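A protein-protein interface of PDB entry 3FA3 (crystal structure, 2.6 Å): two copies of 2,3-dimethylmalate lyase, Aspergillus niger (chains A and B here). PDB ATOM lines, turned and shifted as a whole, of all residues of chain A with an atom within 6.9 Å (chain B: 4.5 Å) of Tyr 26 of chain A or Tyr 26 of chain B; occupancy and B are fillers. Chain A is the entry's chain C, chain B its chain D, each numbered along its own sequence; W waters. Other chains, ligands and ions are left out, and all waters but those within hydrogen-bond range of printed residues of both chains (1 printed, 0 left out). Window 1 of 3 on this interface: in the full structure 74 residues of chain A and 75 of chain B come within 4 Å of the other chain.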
ATOM      1  N   GLY A  24       3.781  -5.425 -29.876  1.00  0.00           N
ATOM      2  CA  GLY A  24       2.503  -5.698 -29.223  1.00  0.00           C
ATOM      3  C   GLY A  24       1.339  -4.722 -29.245  1.00  0.00           C
ATOM      4  O   GLY A  24       1.462  -3.628 -28.800  1.00  0.00           O
ATOM      5  N   VAL A  25       0.206  -5.165 -29.780  1.00  0.00           N
ATOM      6  CA  VAL A  25      -1.054  -4.451 -29.606  1.00  0.00           C
ATOM      7  C   VAL A  25      -2.113  -5.343 -28.967  1.00  0.00           C
ATOM      8  O   VAL A  25      -1.921  -6.552 -28.833  1.00  0.00           O
ATOM      9  CB  VAL A  25      -1.589  -3.916 -30.947  1.00  0.00           C
ATOM     10  CG1 VAL A  25      -0.518  -3.104 -31.660  1.00  0.00           C
ATOM     11  CG2 VAL A  25      -2.066  -5.064 -31.823  1.00  0.00           C
ATOM     12  N   TYR A  26      -3.229  -4.740 -28.573  1.00  0.00           N
ATOM     13  CA  TYR A  26      -4.093  -5.318 -27.549  1.00  0.00           C
ATOM     14  C   TYR A  26      -5.508  -4.755 -27.638  1.00  0.00           C
ATOM     15  O   TYR A  26      -6.328  -4.972 -26.745  1.00  0.00           O
ATOM     16  CB  TYR A  26      -3.513  -5.067 -26.156  1.00  0.00           C
ATOM     17  CG  TYR A  26      -3.591  -3.624 -25.710  1.00  0.00           C
ATOM     18  CD1 TYR A  26      -2.546  -2.744 -25.953  1.00  0.00           C
ATOM     19  CD2 TYR A  26      -4.713  -3.143 -25.047  1.00  0.00           C
ATOM     20  CE1 TYR A  26      -2.613  -1.425 -25.547  1.00  0.00           C
ATOM     21  CE2 TYR A  26      -4.789  -1.824 -24.637  1.00  0.00           C
ATOM     22  CZ  TYR A  26      -3.736  -0.970 -24.890  1.00  0.00           C
ATOM     23  OH  TYR A  26      -3.808   0.343 -24.484  1.00  0.00           O
ATOM     24  N   ASP A  27      -5.786  -4.033 -28.718  1.00  0.00           N
ATOM     25  CA  ASP A  27      -7.128  -3.492 -28.960  1.00  0.00           C
ATOM     26  C   ASP A  27      -7.041  -2.719 -30.272  1.00  0.00           C
ATOM     27  O   ASP A  27      -6.067  -2.834 -30.995  1.00  0.00           O
ATOM     28  CB  ASP A  27      -7.574  -2.567 -27.831  1.00  0.00           C
ATOM     29  CG  ASP A  27      -6.788  -1.301 -27.802  1.00  0.00           C
ATOM     30  OD1 ASP A  27      -5.804  -1.172 -28.562  1.00  0.00           O
ATOM     31  OD2 ASP A  27      -7.165  -0.392 -27.059  1.00  0.00           O
ATOM     32  N   GLY A  28      -8.116  -2.203 -30.733  1.00  0.00           N
ATOM     33  CA  GLY A  28      -8.186  -1.634 -32.032  1.00  0.00           C
ATOM     34  C   GLY A  28      -7.293  -0.445 -32.138  1.00  0.00           C
ATOM     35  O   GLY A  28      -6.645  -0.232 -33.180  1.00  0.00           O
ATOM     36  N   LEU A  29      -7.247   0.362 -31.083  1.00  0.00           N
ATOM     37  CA  LEU A  29      -6.591   1.663 -31.153  1.00  0.00           C
ATOM     38  C   LEU A  29      -5.081   1.501 -31.287  1.00  0.00           C
ATOM     39  O   LEU A  29      -4.466   2.033 -32.211  1.00  0.00           O
ATOM     40  CB  LEU A  29      -6.923   2.497 -29.914  1.00  0.00           C
ATOM     41  CG  LEU A  29      -8.052   3.517 -30.066  1.00  0.00           C
ATOM     42  CD1 LEU A  29      -8.702   3.804 -28.720  1.00  0.00           C
ATOM     43  CD2 LEU A  29      -7.537   4.800 -30.701  1.00  0.00           C
ATOM     44  N   SER A  30      -4.492   0.761 -30.354  1.00  0.00           N
ATOM     45  CA  SER A  30      -3.098   0.366 -30.440  1.00  0.00           C
ATOM     46  C   SER A  30      -2.845  -0.220 -31.825  1.00  0.00           C
ATOM     47  O   SER A  30      -1.847   0.080 -32.464  1.00  0.00           O
ATOM     48  CB  SER A  30      -2.802  -0.644 -29.354  1.00  0.00           C
ATOM     49  OG  SER A  30      -3.782  -1.668 -29.486  1.00  0.00           O
ATOM     50  N   ALA A  31      -3.750  -1.032 -32.328  1.00  0.00           N
ATOM     51  CA  ALA A  31      -3.497  -1.668 -33.607  1.00  0.00           C
ATOM     52  C   ALA A  31      -3.404  -0.602 -34.710  1.00  0.00           C
ATOM     53  O   ALA A  31      -2.423  -0.531 -35.443  1.00  0.00           O
ATOM     54  CB  ALA A  31      -4.566  -2.622 -33.881  1.00  0.00           C
ATOM     55  N   TYR A  43       1.761  -8.093 -33.234  1.00  0.00           N
ATOM     56  CA  TYR A  43       1.545  -9.128 -32.246  1.00  0.00           C
ATOM     57  C   TYR A  43       0.501  -8.720 -31.233  1.00  0.00           C
ATOM     58  O   TYR A  43       0.669  -7.709 -30.573  1.00  0.00           O
ATOM     59  CB  TYR A  43       2.824  -9.426 -31.492  1.00  0.00           C
ATOM     60  CG  TYR A  43       2.644 -10.331 -30.290  1.00  0.00           C
ATOM     61  CD1 TYR A  43       2.347 -11.666 -30.459  1.00  0.00           C
ATOM     62  CD2 TYR A  43       2.790  -9.848 -29.006  1.00  0.00           C
ATOM     63  CE1 TYR A  43       2.207 -12.484 -29.415  1.00  0.00           C
ATOM     64  CE2 TYR A  43       2.642 -10.677 -27.908  1.00  0.00           C
ATOM     65  CZ  TYR A  43       2.349 -11.998 -28.124  1.00  0.00           C
ATOM     66  OH  TYR A  43       2.185 -12.876 -27.063  1.00  0.00           O
ATOM     67  N   MET A  44      -0.554  -9.526 -31.119  1.00  0.00           N
ATOM     68  CA  MET A  44      -1.584  -9.359 -30.135  1.00  0.00           C
ATOM     69  C   MET A  44      -1.130 -10.076 -28.875  1.00  0.00           C
ATOM     70  O   MET A  44      -1.089 -11.302 -28.870  1.00  0.00           O
ATOM     71  CB  MET A  44      -2.936  -9.998 -30.605  1.00  0.00           C
ATOM     72  CG  MET A  44      -4.182  -9.791 -29.618  1.00  0.00           C
ATOM     73  SD  MET A  44      -5.653 -10.828 -29.923  1.00  0.00           S
ATOM     74  CE  MET A  44      -5.118 -12.353 -29.131  1.00  0.00           C
ATOM     75  N   THR A  45      -0.810  -9.312 -27.821  1.00  0.00           N
ATOM     76  CA  THR A  45      -0.492  -9.839 -26.501  1.00  0.00           C
ATOM     77  C   THR A  45      -1.751 -10.393 -25.814  1.00  0.00           C
ATOM     78  O   THR A  45      -2.773  -9.716 -25.784  1.00  0.00           O
ATOM     79  CB  THR A  45       0.115  -8.710 -25.608  1.00  0.00           C
ATOM     80  OG1 THR A  45       0.099  -9.087 -24.224  1.00  0.00           O
ATOM     81  CG2 THR A  45      -0.618  -7.374 -25.796  1.00  0.00           C
ATOM     82  N   GLY A  46      -1.668 -11.617 -25.279  1.00  0.00           N
ATOM     83  CA  GLY A  46      -2.692 -12.184 -24.376  1.00  0.00           C
ATOM     84  C   GLY A  46      -2.809 -11.320 -23.153  1.00  0.00           C
ATOM     85  O   GLY A  46      -3.890 -10.995 -22.684  1.00  0.00           O
ATOM     86  N   ALA A  47      -1.675 -10.929 -22.632  1.00  0.00           N
ATOM     87  CA  ALA A  47      -1.668 -10.138 -21.419  1.00  0.00           C
ATOM     88  C   ALA A  47      -2.479  -8.857 -21.611  1.00  0.00           C
ATOM     89  O   ALA A  47      -3.357  -8.569 -20.801  1.00  0.00           O
ATOM     90  CB  ALA A  47      -0.256  -9.811 -21.031  1.00  0.00           C
ATOM     91  N   GLY A  48      -2.159  -8.136 -22.684  1.00  0.00           N
ATOM     92  CA  GLY A  48      -2.842  -7.006 -23.146  1.00  0.00           C
ATOM     93  C   GLY A  48      -4.258  -7.299 -23.474  1.00  0.00           C
ATOM     94  O   GLY A  48      -5.120  -6.513 -23.088  1.00  0.00           O
ATOM     95  N   THR A  49      -4.577  -8.401 -24.159  1.00  0.00           N
ATOM     96  CA  THR A  49      -6.027  -8.772 -24.261  1.00  0.00           C
ATOM     97  C   THR A  49      -6.771  -8.810 -22.853  1.00  0.00           C
ATOM     98  O   THR A  49      -7.821  -8.163 -22.657  1.00  0.00           O
ATOM     99  CB  THR A  49      -6.283 -10.040 -25.140  1.00  0.00           C
ATOM    100  OG1 THR A  49      -5.752  -9.827 -26.435  1.00  0.00           O
ATOM    101  CG2 THR A  49      -7.783 -10.346 -25.327  1.00  0.00           C
ATOM    102  N   ALA A  50      -6.187  -9.500 -21.880  1.00  0.00           N
ATOM    103  CA  ALA A  50      -6.799  -9.622 -20.568  1.00  0.00           C
ATOM    104  C   ALA A  50      -7.104  -8.275 -19.917  1.00  0.00           C
ATOM    105  O   ALA A  50      -8.173  -8.079 -19.295  1.00  0.00           O
ATOM    106  CB  ALA A  50      -5.897 -10.398 -19.672  1.00  0.00           C
ATOM    107  N   ALA A  51      -6.117  -7.380 -20.051  1.00  0.00           N
ATOM    108  CA  ALA A  51      -6.076  -6.060 -19.431  1.00  0.00           C
ATOM    109  C   ALA A  51      -7.077  -5.080 -20.074  1.00  0.00           C
ATOM    110  O   ALA A  51      -7.803  -4.383 -19.391  1.00  0.00           O
ATOM    111  CB  ALA A  51      -4.722  -5.540 -19.521  1.00  0.00           C
ATOM    112  N   SER A  52      -7.102  -5.027 -21.389  1.00  0.00           N
ATOM    113  CA  SER A  52      -8.034  -4.158 -22.056  1.00  0.00           C
ATOM    114  C   SER A  52      -9.445  -4.763 -22.002  1.00  0.00           C
ATOM    115  O   SER A  52     -10.359  -4.045 -21.664  1.00  0.00           O
ATOM    116  CB  SER A  52      -7.563  -3.799 -23.494  1.00  0.00           C
ATOM    117  OG  SER A  52      -8.598  -3.262 -24.317  1.00  0.00           O
ATOM    118  N   VAL A  53      -9.654  -6.044 -22.312  1.00  0.00           N
ATOM    119  CA  VAL A  53     -11.042  -6.581 -22.353  1.00  0.00           C
ATOM    120  C   VAL A  53     -11.697  -6.703 -20.958  1.00  0.00           C
ATOM    121  O   VAL A  53     -12.926  -6.472 -20.784  1.00  0.00           O
ATOM    122  CB  VAL A  53     -11.131  -7.960 -23.038  1.00  0.00           C
ATOM    123  CG1 VAL A  53     -12.518  -8.485 -23.004  1.00  0.00           C
ATOM    124  CG2 VAL A  53     -10.657  -7.875 -24.478  1.00  0.00           C
ATOM    125  N   ASN A  70     -10.954 -10.757 -30.390  1.00  0.00           N
ATOM    126  CA  ASN A  70      -9.966  -9.782 -30.415  1.00  0.00           C
ATOM    127  C   ASN A  70      -8.957 -10.089 -31.484  1.00  0.00           C
ATOM    128  O   ASN A  70      -8.509  -9.181 -32.195  1.00  0.00           O
ATOM    129  CB  ASN A  70      -9.315  -9.656 -29.062  1.00  0.00           C
ATOM    130  CG  ASN A  70      -8.739  -8.301 -28.865  1.00  0.00           C
ATOM    131  OD1 ASN A  70      -9.375  -7.311 -29.235  1.00  0.00           O
ATOM    132  ND2 ASN A  70      -7.512  -8.232 -28.348  1.00  0.00           N
ATOM    133  N   MET A  73     -10.667  -9.104 -35.111  1.00  0.00           N
ATOM    134  CA  MET A  73     -10.781  -7.698 -35.432  1.00  0.00           C
ATOM    135  C   MET A  73      -9.440  -7.087 -35.757  1.00  0.00           C
ATOM    136  O   MET A  73      -9.307  -6.425 -36.760  1.00  0.00           O
ATOM    137  CB  MET A  73     -11.562  -6.917 -34.344  1.00  0.00           C
ATOM    138  CG  MET A  73     -10.835  -6.264 -33.260  1.00  0.00           C
ATOM    139  SD  MET A  73     -10.074  -4.629 -33.473  1.00  0.00           S
ATOM    140  CE  MET A  73      -9.530  -4.545 -31.770  1.00  0.00           C
ATOM    141  N   ILE A  74      -8.440  -7.341 -34.921  1.00  0.00           N
ATOM    142  CA  ILE A  74      -7.095  -6.823 -35.132  1.00  0.00           C
ATOM    143  C   ILE A  74      -6.587  -7.266 -36.476  1.00  0.00           C
ATOM    144  O   ILE A  74      -5.973  -6.488 -37.170  1.00  0.00           O
ATOM    145  CB  ILE A  74      -6.132  -7.255 -34.030  1.00  0.00           C
ATOM    146  CG1 ILE A  74      -6.255  -6.333 -32.817  1.00  0.00           C
ATOM    147  CG2 ILE A  74      -4.744  -7.104 -34.451  1.00  0.00           C
ATOM    148  CD1 ILE A  74      -5.739  -6.952 -31.456  1.00  0.00           C
ATOM    149  N   PRO A 239       5.495  -7.404 -26.596  1.00  0.00           N
ATOM    150  CA  PRO A 239       4.128  -7.433 -26.007  1.00  0.00           C
ATOM    151  C   PRO A 239       3.613  -6.110 -25.411  1.00  0.00           C
ATOM    152  O   PRO A 239       2.416  -5.747 -25.575  1.00  0.00           O
ATOM    153  CB  PRO A 239       4.278  -8.459 -24.884  1.00  0.00           C
ATOM    154  CG  PRO A 239       5.263  -9.446 -25.479  1.00  0.00           C
ATOM    155  CD  PRO A 239       6.269  -8.612 -26.232  1.00  0.00           C
ATOM    156  N   ALA A 241       4.788  -2.931 -25.984  1.00  0.00           N
ATOM    157  CA  ALA A 241       5.003  -1.762 -26.826  1.00  0.00           C
ATOM    158  C   ALA A 241       3.985  -0.667 -26.739  1.00  0.00           C
ATOM    159  O   ALA A 241       4.371   0.457 -26.706  1.00  0.00           O
ATOM    160  CB  ALA A 241       5.087  -2.213 -28.239  1.00  0.00           C
ATOM    161  N   ALA A 242       2.697  -0.968 -26.793  1.00  0.00           N
ATOM    162  CA  ALA A 242       1.666   0.068 -26.666  1.00  0.00           C
ATOM    163  C   ALA A 242       1.186   0.117 -25.243  1.00  0.00           C
ATOM    164  O   ALA A 242       0.840   1.158 -24.735  1.00  0.00           O
ATOM    165  CB  ALA A 242       0.519  -0.208 -27.545  1.00  0.00           C
ATOM    166  N   LEU A 243       1.146  -1.012 -24.582  1.00  0.00           N
ATOM    167  CA  LEU A 243       0.469  -1.023 -23.332  1.00  0.00           C
ATOM    168  C   LEU A 243       1.212  -0.218 -22.189  1.00  0.00           C
ATOM    169  O   LEU A 243       0.590   0.649 -21.478  1.00  0.00           O
ATOM    170  CB  LEU A 243       0.163  -2.474 -22.993  1.00  0.00           C
ATOM    171  CG  LEU A 243      -0.722  -2.806 -21.817  1.00  0.00           C
ATOM    172  CD1 LEU A 243      -1.405  -4.088 -22.103  1.00  0.00           C
ATOM    173  CD2 LEU A 243       0.185  -2.953 -20.610  1.00  0.00           C
ATOM    174  N   GLY A 244       2.509  -0.491 -22.010  1.00  0.00           N
ATOM    175  CA  GLY A 244       3.312   0.273 -21.076  1.00  0.00           C
ATOM    176  C   GLY A 244       3.085   1.762 -21.245  1.00  0.00           C
ATOM    177  O   GLY A 244       2.726   2.462 -20.280  1.00  0.00           O
ATOM    178  N   ALA A 246       0.732   3.417 -22.861  1.00  0.00           N
ATOM    179  CA  ALA A 246      -0.638   3.883 -22.621  1.00  0.00           C
ATOM    180  C   ALA A 246      -0.938   3.938 -21.123  1.00  0.00           C
ATOM    181  O   ALA A 246      -1.708   4.787 -20.668  1.00  0.00           O
ATOM    182  CB  ALA A 246      -1.606   3.008 -23.263  1.00  0.00           C
ATOM    183  N   VAL A 247      -0.340   3.040 -20.349  1.00  0.00           N
ATOM    184  CA  VAL A 247      -0.624   3.040 -18.977  1.00  0.00           C
ATOM    185  C   VAL A 247       0.053   4.280 -18.358  1.00  0.00           C
ATOM    186  O   VAL A 247      -0.524   4.975 -17.496  1.00  0.00           O
ATOM    187  CB  VAL A 247      -0.154   1.772 -18.377  1.00  0.00           C
ATOM    188  CG1 VAL A 247      -0.183   1.876 -16.857  1.00  0.00           C
ATOM    189  CG2 VAL A 247      -1.060   0.620 -18.821  1.00  0.00           C
ATOM    190  N   MET A 250      -1.894   7.585 -19.526  1.00  0.00           N
ATOM    191  CA  MET A 250      -3.246   7.719 -18.983  1.00  0.00           C
ATOM    192  C   MET A 250      -3.175   8.046 -17.487  1.00  0.00           C
ATOM    193  O   MET A 250      -3.953   8.822 -16.981  1.00  0.00           O
ATOM    194  CB  MET A 250      -4.072   6.463 -19.239  1.00  0.00           C
ATOM    195  CG  MET A 250      -4.210   6.108 -20.692  1.00  0.00           C
ATOM    196  SD  MET A 250      -5.477   4.848 -20.880  1.00  0.00           S
ATOM    197  CE  MET A 250      -4.686   3.261 -20.553  1.00  0.00           C
ATOM    198  N   VAL B  25     -13.630   6.669 -19.685  1.00  0.00           N
ATOM    199  CA  VAL B  25     -12.927   5.395 -20.004  1.00  0.00           C
ATOM    200  C   VAL B  25     -13.553   4.516 -21.161  1.00  0.00           C
ATOM    201  O   VAL B  25     -14.771   4.588 -21.457  1.00  0.00           O
ATOM    202  CB  VAL B  25     -12.623   4.518 -18.716  1.00  0.00           C
ATOM    203  CG1 VAL B  25     -11.949   5.331 -17.656  1.00  0.00           C
ATOM    204  CG2 VAL B  25     -13.865   3.942 -18.168  1.00  0.00           C
ATOM    205  N   TYR B  26     -12.703   3.660 -21.743  1.00  0.00           N
ATOM    206  CA  TYR B  26     -13.028   2.856 -22.898  1.00  0.00           C
ATOM    207  C   TYR B  26     -12.661   1.359 -22.837  1.00  0.00           C
ATOM    208  O   TYR B  26     -12.988   0.636 -23.778  1.00  0.00           O
ATOM    209  CB  TYR B  26     -12.398   3.474 -24.141  1.00  0.00           C
ATOM    210  CG  TYR B  26     -10.893   3.399 -24.183  1.00  0.00           C
ATOM    211  CD1 TYR B  26     -10.080   4.424 -23.656  1.00  0.00           C
ATOM    212  CD2 TYR B  26     -10.264   2.272 -24.738  1.00  0.00           C
ATOM    213  CE1 TYR B  26      -8.675   4.330 -23.712  1.00  0.00           C
ATOM    214  CE2 TYR B  26      -8.874   2.153 -24.782  1.00  0.00           C
ATOM    215  CZ  TYR B  26      -8.088   3.181 -24.295  1.00  0.00           C
ATOM    216  OH  TYR B  26      -6.741   2.983 -24.388  1.00  0.00           O
ATOM    217  N   ASP B  27     -12.015   0.881 -21.776  1.00  0.00           N
ATOM    218  CA  ASP B  27     -11.600  -0.525 -21.659  1.00  0.00           C
ATOM    219  C   ASP B  27     -11.110  -0.824 -20.239  1.00  0.00           C
ATOM    220  O   ASP B  27     -11.129   0.051 -19.358  1.00  0.00           O
ATOM    221  CB  ASP B  27     -10.467  -0.826 -22.640  1.00  0.00           C
ATOM    222  CG  ASP B  27      -9.151  -0.241 -22.197  1.00  0.00           C
ATOM    223  OD1 ASP B  27      -9.106   0.711 -21.357  1.00  0.00           O
ATOM    224  OD2 ASP B  27      -8.136  -0.740 -22.691  1.00  0.00           O
ATOM    225  N   LEU B  29      -8.240  -1.101 -18.854  1.00  0.00           N
ATOM    226  CA  LEU B  29      -7.089  -0.372 -18.307  1.00  0.00           C
ATOM    227  C   LEU B  29      -7.346   1.066 -17.908  1.00  0.00           C
ATOM    228  O   LEU B  29      -7.015   1.455 -16.780  1.00  0.00           O
ATOM    229  CB  LEU B  29      -5.916  -0.381 -19.258  1.00  0.00           C
ATOM    230  CG  LEU B  29      -4.964  -1.537 -19.112  1.00  0.00           C
ATOM    231  CD1 LEU B  29      -4.400  -1.764 -20.524  1.00  0.00           C
ATOM    232  CD2 LEU B  29      -3.923  -1.055 -18.184  1.00  0.00           C
ATOM    233  N   SER B  30      -7.901   1.845 -18.843  1.00  0.00           N
ATOM    234  CA  SER B  30      -8.374   3.221 -18.589  1.00  0.00           C
ATOM    235  C   SER B  30      -9.272   3.260 -17.340  1.00  0.00           C
ATOM    236  O   SER B  30      -9.286   4.249 -16.577  1.00  0.00           O
ATOM    237  CB  SER B  30      -9.178   3.711 -19.796  1.00  0.00           C
ATOM    238  OG  SER B  30     -10.189   2.778 -20.218  1.00  0.00           O
ATOM    239  N   THR B  45     -17.347   5.701 -22.618  1.00  0.00           N
ATOM    240  CA  THR B  45     -17.644   6.315 -23.942  1.00  0.00           C
ATOM    241  C   THR B  45     -18.076   5.304 -25.075  1.00  0.00           C
ATOM    242  O   THR B  45     -17.447   4.249 -25.280  1.00  0.00           O
ATOM    243  CB  THR B  45     -16.466   7.233 -24.373  1.00  0.00           C
ATOM    244  OG1 THR B  45     -16.484   7.443 -25.786  1.00  0.00           O
ATOM    245  CG2 THR B  45     -15.169   6.621 -23.975  1.00  0.00           C
ATOM    246  N   GLY B  48     -15.252   5.612 -27.510  1.00  0.00           N
ATOM    247  CA  GLY B  48     -14.092   4.881 -27.098  1.00  0.00           C
ATOM    248  C   GLY B  48     -14.298   3.404 -27.181  1.00  0.00           C
ATOM    249  O   GLY B  48     -13.359   2.675 -27.528  1.00  0.00           O
ATOM    250  N   THR B  49     -15.513   2.930 -26.882  1.00  0.00           N
ATOM    251  CA  THR B  49     -15.794   1.496 -27.113  1.00  0.00           C
ATOM    252  C   THR B  49     -15.481   1.061 -28.608  1.00  0.00           C
ATOM    253  O   THR B  49     -14.770   0.044 -28.875  1.00  0.00           O
ATOM    254  CB  THR B  49     -17.203   1.097 -26.661  1.00  0.00           C
ATOM    255  OG1 THR B  49     -17.448   1.621 -25.357  1.00  0.00           O
ATOM    256  CG2 THR B  49     -17.296  -0.360 -26.531  1.00  0.00           C
ATOM    257  N   SER B  52     -11.736   0.952 -29.225  1.00  0.00           N
ATOM    258  CA  SER B  52     -10.950  -0.081 -28.660  1.00  0.00           C
ATOM    259  C   SER B  52     -11.410  -1.463 -29.101  1.00  0.00           C
ATOM    260  O   SER B  52     -10.573  -2.279 -29.434  1.00  0.00           O
ATOM    261  CB  SER B  52     -10.917   0.051 -27.163  1.00  0.00           C
ATOM    262  OG  SER B  52     -10.154  -1.020 -26.676  1.00  0.00           O
ATOM    263  N   ASN B  70     -18.899  -4.382 -22.468  1.00  0.00           N
ATOM    264  CA  ASN B  70     -17.926  -3.430 -22.081  1.00  0.00           C
ATOM    265  C   ASN B  70     -18.456  -2.670 -20.880  1.00  0.00           C
ATOM    266  O   ASN B  70     -17.766  -2.501 -19.913  1.00  0.00           O
ATOM    267  CB  ASN B  70     -17.554  -2.495 -23.268  1.00  0.00           C
ATOM    268  CG  ASN B  70     -16.170  -1.852 -23.104  1.00  0.00           C
ATOM    269  OD1 ASN B  70     -15.227  -2.510 -22.680  1.00  0.00           O
ATOM    270  ND2 ASN B  70     -16.057  -0.540 -23.425  1.00  0.00           N
ATOM    271  N   ALA B 242      -9.052   9.486 -21.191  1.00  0.00           N
ATOM    272  CA  ALA B 242      -8.081   8.427 -21.357  1.00  0.00           C
ATOM    273  C   ALA B 242      -7.596   8.263 -22.826  1.00  0.00           C
ATOM    274  O   ALA B 242      -6.397   8.259 -23.149  1.00  0.00           O
ATOM    275  CB  ALA B 242      -8.701   7.164 -20.868  1.00  0.00           C
ATOM    276  N   LEU B 243      -8.584   8.158 -23.695  1.00  0.00           N
ATOM    277  CA  LEU B 243      -8.394   7.900 -25.109  1.00  0.00           C
ATOM    278  C   LEU B 243      -7.431   8.833 -25.774  1.00  0.00           C
ATOM    279  O   LEU B 243      -6.705   8.402 -26.635  1.00  0.00           O
ATOM    280  CB  LEU B 243      -9.730   8.038 -25.853  1.00  0.00           C
ATOM    281  CG  LEU B 243      -9.741   7.172 -27.068  1.00  0.00           C
ATOM    282  CD1 LEU B 243     -10.722   6.148 -26.728  1.00  0.00           C
ATOM    283  CD2 LEU B 243     -10.092   7.956 -28.311  1.00  0.00           C
ATOM    284  N   ALA B 246      -3.702   8.346 -24.533  1.00  0.00           N
ATOM    285  CA  ALA B 246      -3.282   7.029 -24.885  1.00  0.00           C
ATOM    286  C   ALA B 246      -2.917   6.998 -26.332  1.00  0.00           C
ATOM    287  O   ALA B 246      -1.930   6.376 -26.676  1.00  0.00           O
ATOM    288  CB  ALA B 246      -4.386   6.016 -24.569  1.00  0.00           C
ATOM    289  N   MET B 250       1.008   6.214 -27.562  1.00  0.00           N
ATOM    290  CA  MET B 250       1.279   4.971 -28.313  1.00  0.00           C
ATOM    291  C   MET B 250       1.950   5.310 -29.628  1.00  0.00           C
ATOM    292  O   MET B 250       2.911   4.644 -30.043  1.00  0.00           O
ATOM    293  CB  MET B 250       0.017   4.182 -28.559  1.00  0.00           C
ATOM    294  CG  MET B 250      -0.664   3.662 -27.264  1.00  0.00           C
ATOM    295  SD  MET B 250      -1.961   2.436 -27.496  1.00  0.00           S
ATOM    296  CE  MET B 250      -3.445   3.391 -27.790  1.00  0.00           C
HETATM  297  O   HOH W   1     -10.900  -3.454 -25.643  1.00  0.00           O
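Tyr 26 of chain B touches its own counterpart, Tyr 26 of chain A.
Asp 27 of chain A touches Ser 52 of chain B, and with the chains exchanged Ser 52 of chain A touches Asp 27 of chain B.
Ser 30 of chain A touches Met 250 of chain B, and with the chains exchanged Met 250 of chain A touches Ser 30 of chain B.
Ala 242 of chain A touches Met 250 of chain B, and with the chains exchanged Met 250 of chain A touches Ala 242 of chain B.
Of the 15 pairs that touch across the chains among the printed residues, 8 have their exchanged pair printed and touching as well.
Water W1 lies within hydrogen-bond range of the side-chain hydroxyl of Ser 52 of chain A and the side-chain hydroxyl of Ser 52 of chain B.
OH of Tyr 26 of chain B touches OH of Tyr 26 of chain A (3.9 Å).
Leu 243 of chain B touches Leu 29 of chain A.
Ser 30 of chain A touches Met 250 of chain B (CB to SD, 3.7 Å).
OG of Ser 52 of chain A touches OG of Ser 52 of chain B, 3.6 Å away.
Ser 52 of chain B touches Met 73 of chain A (O to CE, 3.4 Å).
SD of Met 250 of chain B touches CB of Ala 242 of chain A, at 3.6 Å.
Val 247 of chain A touches Leu 29 of chain B (CG2 to CD2, 3.4 Å).
N of Ser 30 of chain B touches CE of Met 250 of chain A, 3.9 Å away.
CG of Met 250 of chain A touches O of Ala 242 of chain B, at 3.9 Å.
Ala 246 of chain B touches Met 250 of chain A.
Hydrophobic or aromatic side chains of chain B that line the printed part of chain A: Tyr 26, Leu 29, Ala 242, Leu 243, Ala 246 and Met 250.
Along chain A the printed residues that touch a printed residue of chain B span positions 26 to 250.
Among the printed residues, 15 pairs touch across the chains.
The side-chain carboxylate (OD2) of Asp 27 of chain A sits at hydrogen-bond distance from the side-chain hydroxyl (OG) of Ser 52 of chain B, 3.1 Å away.
The backbone NH of Gly 28 of chain A lies within hydrogen-bond range of the backbone carbonyl oxygen of Ser 52 of chain B (2.8 Å).
O of Ala 51 of chain A lies within hydrogen-bond range of N of Leu 29 of chain B (3.4 Å).
OG of Ser 52 of chain A sits at hydrogen-bond distance from OD2 of Asp 27 of chain B, 3.0 Å away.
The backbone NH (N) of Tyr 26 of chain A sits at hydrogen-bond distance from the side-chain hydroxyl (OG) of Ser 30 of chain A (3.3 Å).
The side-chain carboxylate (OD1) of Asp 27 of chain A lies close to the backbone NH (N) of Leu 29 of chain A.
The backbone NH of Ser 30 of chain A is in hydrogen-bond range of the side-chain carboxylate of Asp 27 of chain A (2.9 Å).
The side-chain amide nitrogen (ND2) of Asn 70 of chain B is in hydrogen-bond range of the backbone carbonyl oxygen (O) of Tyr 26 of chain B (3.3 Å).
The side-chain carboxylate (OD1) of Asp 27 of chain B sits close to the backbone NH (N) of Leu 29 of chain B (3.2 Å).
OD1 of Asp 27 of chain B lies within hydrogen-bond range of OG of Ser 30 of chain B, 2.6 Å away.
Of the printed residues of chain B, Tyr 26 of chain A touches Tyr 26 (3.9 Å).
Of chain A, only Tyr 26 and Asp 27 come within 4 Å of Tyr 26 of chain B.
Of the printed residues of chain B, Met 250 of chain A touches Ser 30, Ala 242 and Ala 246.
Of the printed residues of chain A, Ser 52 of chain B touches Asp 27, Gly 28, Ser 52 and Met 73.
Leu 243 of chain A touches none of the printed residues of chain B.
The nearest residue of chain B that does not touch Tyr 26 of chain A is Asp 27 of chain B (4.02 Å).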
